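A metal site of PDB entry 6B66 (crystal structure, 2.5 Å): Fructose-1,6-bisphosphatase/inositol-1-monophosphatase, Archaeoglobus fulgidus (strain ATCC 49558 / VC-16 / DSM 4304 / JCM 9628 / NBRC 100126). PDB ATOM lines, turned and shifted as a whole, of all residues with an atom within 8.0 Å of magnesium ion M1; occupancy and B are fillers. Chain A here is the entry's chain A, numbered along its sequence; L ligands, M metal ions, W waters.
N of Glu 67 sits at hydrogen-bond distance from O of Leu 81, at 3.5 Å.
The side-chain carboxylate of Glu 67 sits close to the side-chain hydroxyl of Thr 40, 3.4 Å away.
NH1 of Arg 197 lies within salt-bridge range of OE1 of Glu 67 (3.3 Å).
The backbone NH (N) of Asp 38 lies within hydrogen-bond range of the backbone carbonyl oxygen (O) of Glu 67 (3.3 Å).
OG1 of Thr 87 lies close to O of Leu 84, at 3.2 Å.
Magnesium ion M1 is bound by water W1 (2.1 Å), the side-chain carboxylate (OE2) of Glu 67 (2.1 Å), the side-chain carboxylate (OD1) of Asp 82 (2.1 Å), the backbone carbonyl oxygen (O) of Leu 84 (2.2 Å), an oxygen (O2) of the ligand (2.3 Å) and an oxygen (O3) of the ligand (2.6 Å).
Water W1 lies within hydrogen-bond range of the side-chain carboxylate (OE2) of Glu 68, the side-chain carboxylate (OD1) of Asp 46 and the backbone NH (N) of Leu 84.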
ATOM      1  N   ASP A  38      30.761  -0.369 -19.622  1.00  0.00           N
ATOM      2  CA  ASP A  38      29.913   0.689 -20.182  1.00  0.00           C
ATOM      3  C   ASP A  38      30.519   2.060 -19.979  1.00  0.00           C
ATOM      4  O   ASP A  38      30.048   3.045 -20.559  1.00  0.00           O
ATOM      5  CB  ASP A  38      28.527   0.660 -19.546  1.00  0.00           C
ATOM      6  CG  ASP A  38      28.524   1.208 -18.133  1.00  0.00           C
ATOM      7  OD1 ASP A  38      29.230   0.646 -17.265  1.00  0.00           O
ATOM      8  OD2 ASP A  38      27.841   2.212 -17.876  1.00  0.00           O
ATOM      9  N   THR A  40      30.772   3.394 -16.729  1.00  0.00           N
ATOM     10  CA  THR A  40      30.325   3.929 -15.440  1.00  0.00           C
ATOM     11  C   THR A  40      30.713   2.975 -14.321  1.00  0.00           C
ATOM     12  O   THR A  40      30.863   1.763 -14.560  1.00  0.00           O
ATOM     13  CB  THR A  40      28.802   4.165 -15.393  1.00  0.00           C
ATOM     14  OG1 THR A  40      28.119   2.903 -15.503  1.00  0.00           O
ATOM     15  CG2 THR A  40      28.369   5.134 -16.506  1.00  0.00           C
ATOM     16  N   PRO A  41      30.881   3.502 -13.094  1.00  0.00           N
ATOM     17  CA  PRO A  41      31.272   2.651 -11.960  1.00  0.00           C
ATOM     18  C   PRO A  41      30.380   1.411 -11.812  1.00  0.00           C
ATOM     19  O   PRO A  41      29.183   1.495 -12.078  1.00  0.00           O
ATOM     20  CB  PRO A  41      31.073   3.585 -10.751  1.00  0.00           C
ATOM     21  CG  PRO A  41      31.289   4.939 -11.303  1.00  0.00           C
ATOM     22  CD  PRO A  41      30.721   4.911 -12.690  1.00  0.00           C
ATOM     23  N   ASP A  46      25.741  -4.086  -8.345  1.00  0.00           N
ATOM     24  CA  ASP A  46      25.821  -4.430  -9.775  1.00  0.00           C
ATOM     25  C   ASP A  46      26.578  -5.733  -9.986  1.00  0.00           C
ATOM     26  O   ASP A  46      26.108  -6.625 -10.708  1.00  0.00           O
ATOM     27  CB  ASP A  46      26.493  -3.324 -10.599  1.00  0.00           C
ATOM     28  CG  ASP A  46      25.684  -2.034 -10.631  1.00  0.00           C
ATOM     29  OD1 ASP A  46      24.450  -2.108 -10.899  1.00  0.00           O
ATOM     30  OD2 ASP A  46      26.281  -0.955 -10.389  1.00  0.00           O
ATOM     31  N   ALA A  49      24.701  -8.888  -8.863  1.00  0.00           N
ATOM     32  CA  ALA A  49      23.598  -9.129  -9.783  1.00  0.00           C
ATOM     33  C   ALA A  49      24.124  -9.771 -11.043  1.00  0.00           C
ATOM     34  O   ALA A  49      23.663 -10.853 -11.446  1.00  0.00           O
ATOM     35  CB  ALA A  49      22.848  -7.839 -10.115  1.00  0.00           C
ATOM     36  N   GLU A  50      25.107  -9.133 -11.658  1.00  0.00           N
ATOM     37  CA  GLU A  50      25.625  -9.624 -12.922  1.00  0.00           C
ATOM     38  C   GLU A  50      26.235 -11.007 -12.785  1.00  0.00           C
ATOM     39  O   GLU A  50      26.016 -11.863 -13.650  1.00  0.00           O
ATOM     40  CB  GLU A  50      26.616  -8.660 -13.551  1.00  0.00           C
ATOM     41  CG  GLU A  50      26.987  -9.048 -14.977  1.00  0.00           C
ATOM     42  CD  GLU A  50      27.897  -8.031 -15.649  1.00  0.00           C
ATOM     43  OE1 GLU A  50      27.411  -7.249 -16.497  1.00  0.00           O
ATOM     44  OE2 GLU A  50      29.107  -8.008 -15.349  1.00  0.00           O
ATOM     45  N   THR A  66      26.022  -6.898 -21.713  1.00  0.00           N
ATOM     46  CA  THR A  66      25.604  -6.536 -20.370  1.00  0.00           C
ATOM     47  C   THR A  66      26.432  -5.372 -19.846  1.00  0.00           C
ATOM     48  O   THR A  66      27.578  -5.174 -20.244  1.00  0.00           O
ATOM     49  CB  THR A  66      25.733  -7.755 -19.432  1.00  0.00           C
ATOM     50  OG1 THR A  66      25.440  -7.352 -18.087  1.00  0.00           O
ATOM     51  CG2 THR A  66      27.153  -8.325 -19.505  1.00  0.00           C
ATOM     52  N   GLU A  67      25.857  -4.600 -18.934  1.00  0.00           N
ATOM     53  CA  GLU A  67      26.419  -3.311 -18.568  1.00  0.00           C
ATOM     54  C   GLU A  67      27.816  -3.359 -17.958  1.00  0.00           C
ATOM     55  O   GLU A  67      28.694  -2.593 -18.340  1.00  0.00           O
ATOM     56  CB  GLU A  67      25.501  -2.541 -17.624  1.00  0.00           C
ATOM     57  CG  GLU A  67      26.062  -1.191 -17.259  1.00  0.00           C
ATOM     58  CD  GLU A  67      25.278  -0.508 -16.176  1.00  0.00           C
ATOM     59  OE1 GLU A  67      25.789   0.498 -15.606  1.00  0.00           O
ATOM     60  OE2 GLU A  67      24.150  -1.000 -15.902  1.00  0.00           O
ATOM     61  N   GLU A  68      28.028  -4.256 -16.997  1.00  0.00           N
ATOM     62  CA  GLU A  68      29.309  -4.260 -16.272  1.00  0.00           C
ATOM     63  C   GLU A  68      30.419  -4.954 -17.070  1.00  0.00           C
ATOM     64  O   GLU A  68      31.510  -4.405 -17.222  1.00  0.00           O
ATOM     65  CB  GLU A  68      29.172  -4.853 -14.855  1.00  0.00           C
ATOM     66  CG  GLU A  68      27.941  -4.394 -14.070  1.00  0.00           C
ATOM     67  CD  GLU A  68      27.789  -2.878 -14.036  1.00  0.00           C
ATOM     68  OE1 GLU A  68      28.822  -2.164 -14.069  1.00  0.00           O
ATOM     69  OE2 GLU A  68      26.640  -2.386 -13.972  1.00  0.00           O
ATOM     70  N   LEU A  81      21.362  -7.474 -21.421  1.00  0.00           N
ATOM     71  CA  LEU A  81      21.195  -7.661 -19.971  1.00  0.00           C
ATOM     72  C   LEU A  81      21.541  -6.415 -19.172  1.00  0.00           C
ATOM     73  O   LEU A  81      22.669  -5.902 -19.239  1.00  0.00           O
ATOM     74  CB  LEU A  81      22.060  -8.836 -19.486  1.00  0.00           C
ATOM     75  CG  LEU A  81      22.205  -9.026 -17.968  1.00  0.00           C
ATOM     76  CD1 LEU A  81      20.860  -9.307 -17.270  1.00  0.00           C
ATOM     77  CD2 LEU A  81      23.185 -10.152 -17.682  1.00  0.00           C
ATOM     78  N   ASP A  82      20.570  -5.908 -18.438  1.00  0.00           N
ATOM     79  CA  ASP A  82      20.872  -4.958 -17.369  1.00  0.00           C
ATOM     80  C   ASP A  82      20.680  -5.757 -16.090  1.00  0.00           C
ATOM     81  O   ASP A  82      19.553  -6.021 -15.679  1.00  0.00           O
ATOM     82  CB  ASP A  82      19.945  -3.739 -17.422  1.00  0.00           C
ATOM     83  CG  ASP A  82      20.509  -2.532 -16.656  1.00  0.00           C
ATOM     84  OD1 ASP A  82      21.468  -2.713 -15.851  1.00  0.00           O
ATOM     85  OD2 ASP A  82      19.991  -1.415 -16.854  1.00  0.00           O
ATOM     86  N   PRO A  83      21.789  -6.177 -15.476  1.00  0.00           N
ATOM     87  CA  PRO A  83      21.696  -7.062 -14.312  1.00  0.00           C
ATOM     88  C   PRO A  83      21.048  -6.337 -13.135  1.00  0.00           C
ATOM     89  O   PRO A  83      20.398  -6.959 -12.290  1.00  0.00           O
ATOM     90  CB  PRO A  83      23.155  -7.406 -14.015  1.00  0.00           C
ATOM     91  CG  PRO A  83      23.934  -6.265 -14.558  1.00  0.00           C
ATOM     92  CD  PRO A  83      23.181  -5.754 -15.751  1.00  0.00           C
ATOM     93  N   LEU A  84      21.210  -5.024 -13.093  1.00  0.00           N
ATOM     94  CA  LEU A  84      20.563  -4.212 -12.072  1.00  0.00           C
ATOM     95  C   LEU A  84      20.296  -2.827 -12.652  1.00  0.00           C
ATOM     96  O   LEU A  84      21.224  -2.044 -12.842  1.00  0.00           O
ATOM     97  CB  LEU A  84      21.443  -4.106 -10.821  1.00  0.00           C
ATOM     98  CG  LEU A  84      20.895  -3.255  -9.670  1.00  0.00           C
ATOM     99  CD1 LEU A  84      19.514  -3.752  -9.243  1.00  0.00           C
ATOM    100  CD2 LEU A  84      21.867  -3.212  -8.477  1.00  0.00           C
ATOM    101  N   ASP A  85      19.030  -2.542 -12.939  1.00  0.00           N
ATOM    102  CA  ASP A  85      18.641  -1.269 -13.520  1.00  0.00           C
ATOM    103  C   ASP A  85      17.949  -0.498 -12.420  1.00  0.00           C
ATOM    104  O   ASP A  85      17.018  -1.006 -11.817  1.00  0.00           O
ATOM    105  CB  ASP A  85      17.702  -1.480 -14.704  1.00  0.00           C
ATOM    106  CG  ASP A  85      17.320  -0.174 -15.377  1.00  0.00           C
ATOM    107  OD1 ASP A  85      18.235   0.514 -15.892  1.00  0.00           O
ATOM    108  OD2 ASP A  85      16.112   0.168 -15.391  1.00  0.00           O
ATOM    109  N   GLY A  86      18.429   0.716 -12.161  1.00  0.00           N
ATOM    110  CA  GLY A  86      17.981   1.453 -10.991  1.00  0.00           C
ATOM    111  C   GLY A  86      18.914   1.277  -9.792  1.00  0.00           C
ATOM    112  O   GLY A  86      18.486   1.343  -8.641  1.00  0.00           O
ATOM    113  N   THR A  87      20.201   1.051 -10.074  1.00  0.00           N
ATOM    114  CA  THR A  87      21.190   0.788  -9.019  1.00  0.00           C
ATOM    115  C   THR A  87      21.139   1.803  -7.852  1.00  0.00           C
ATOM    116  O   THR A  87      21.259   1.420  -6.681  1.00  0.00           O
ATOM    117  CB  THR A  87      22.627   0.710  -9.584  1.00  0.00           C
ATOM    118  OG1 THR A  87      22.700  -0.288 -10.626  1.00  0.00           O
ATOM    119  CG2 THR A  87      23.620   0.341  -8.480  1.00  0.00           C
ATOM    120  N   SER A  98      15.342  -3.246 -10.933  1.00  0.00           N
ATOM    121  CA  SER A  98      14.965  -4.440 -11.669  1.00  0.00           C
ATOM    122  C   SER A  98      16.150  -5.089 -12.342  1.00  0.00           C
ATOM    123  O   SER A  98      17.207  -4.483 -12.481  1.00  0.00           O
ATOM    124  CB  SER A  98      13.958  -4.073 -12.771  1.00  0.00           C
ATOM    125  OG  SER A  98      12.735  -3.615 -12.212  1.00  0.00           O
ATOM    126  N   VAL A  99      15.963  -6.332 -12.764  1.00  0.00           N
ATOM    127  CA  VAL A  99      16.851  -6.937 -13.738  1.00  0.00           C
ATOM    128  C   VAL A  99      16.055  -7.005 -15.052  1.00  0.00           C
ATOM    129  O   VAL A  99      14.843  -7.273 -15.053  1.00  0.00           O
ATOM    130  CB  VAL A  99      17.316  -8.324 -13.300  1.00  0.00           C
ATOM    131  CG1 VAL A  99      16.125  -9.222 -13.014  1.00  0.00           C
ATOM    132  CG2 VAL A  99      18.209  -8.938 -14.368  1.00  0.00           C
ATOM    133  N   ARG A 197      21.203   3.099 -22.840  1.00  0.00           N
ATOM    134  CA  ARG A 197      21.928   2.074 -23.579  1.00  0.00           C
ATOM    135  C   ARG A 197      20.971   0.927 -23.924  1.00  0.00           C
ATOM    136  O   ARG A 197      19.867   0.843 -23.374  1.00  0.00           O
ATOM    137  CB  ARG A 197      23.129   1.627 -22.769  1.00  0.00           C
ATOM    138  CG  ARG A 197      24.099   2.779 -22.500  1.00  0.00           C
ATOM    139  CD  ARG A 197      24.766   2.688 -21.142  1.00  0.00           C
ATOM    140  NE  ARG A 197      23.813   2.756 -20.038  1.00  0.00           N
ATOM    141  CZ  ARG A 197      24.075   2.310 -18.818  1.00  0.00           C
ATOM    142  NH1 ARG A 197      25.256   1.763 -18.569  1.00  0.00           N
ATOM    143  NH2 ARG A 197      23.163   2.411 -17.854  1.00  0.00           N
ATOM    144  N   TYR A 199      20.638  -2.064 -23.155  1.00  0.00           N
ATOM    145  CA  TYR A 199      20.179  -2.969 -22.098  1.00  0.00           C
ATOM    146  C   TYR A 199      19.243  -2.280 -21.120  1.00  0.00           C
ATOM    147  O   TYR A 199      18.479  -2.955 -20.415  1.00  0.00           O
ATOM    148  CB  TYR A 199      21.347  -3.654 -21.374  1.00  0.00           C
ATOM    149  CG  TYR A 199      22.517  -2.739 -21.153  1.00  0.00           C
ATOM    150  CD1 TYR A 199      23.659  -2.846 -21.945  1.00  0.00           C
ATOM    151  CD2 TYR A 199      22.490  -1.749 -20.176  1.00  0.00           C
ATOM    152  CE1 TYR A 199      24.737  -2.001 -21.764  1.00  0.00           C
ATOM    153  CE2 TYR A 199      23.562  -0.904 -19.986  1.00  0.00           C
ATOM    154  CZ  TYR A 199      24.683  -1.037 -20.794  1.00  0.00           C
ATOM    155  OH  TYR A 199      25.766  -0.204 -20.633  1.00  0.00           O
ATOM    156  N   ASP A 200      19.277  -0.958 -21.093  1.00  0.00           N
ATOM    157  CA  ASP A 200      18.286  -0.178 -20.334  1.00  0.00           C
ATOM    158  C   ASP A 200      16.886  -0.264 -20.947  1.00  0.00           C
ATOM    159  O   ASP A 200      15.893  -0.394 -20.237  1.00  0.00           O
ATOM    160  CB  ASP A 200      18.691   1.296 -20.304  1.00  0.00           C
ATOM    161  CG  ASP A 200      19.948   1.542 -19.484  1.00  0.00           C
ATOM    162  OD1 ASP A 200      20.024   1.005 -18.357  1.00  0.00           O
ATOM    163  OD2 ASP A 200      20.843   2.267 -20.001  1.00  0.00           O
HETATM  164  S1  LIG L   1      21.969   1.279 -14.318  1.00  0.00           S
HETATM  165  O1  LIG L   1      22.727   2.353 -14.986  1.00  0.00           O
HETATM  166  O2  LIG L   1      22.911   0.464 -13.509  1.00  0.00           O
HETATM  167  O3  LIG L   1      21.281   0.454 -15.336  1.00  0.00           O
HETATM  168  O4  LIG L   1      20.955   1.885 -13.431  1.00  0.00           O
HETATM  169 MG    MG M   1      22.641  -1.550 -14.483  1.00  0.00          MG
HETATM  170 MG    MG M   2      28.569   0.691 -15.036  1.00  0.00          MG
HETATM  171  O   HOH W   1      23.909  -2.943 -13.577  1.00  0.00           O
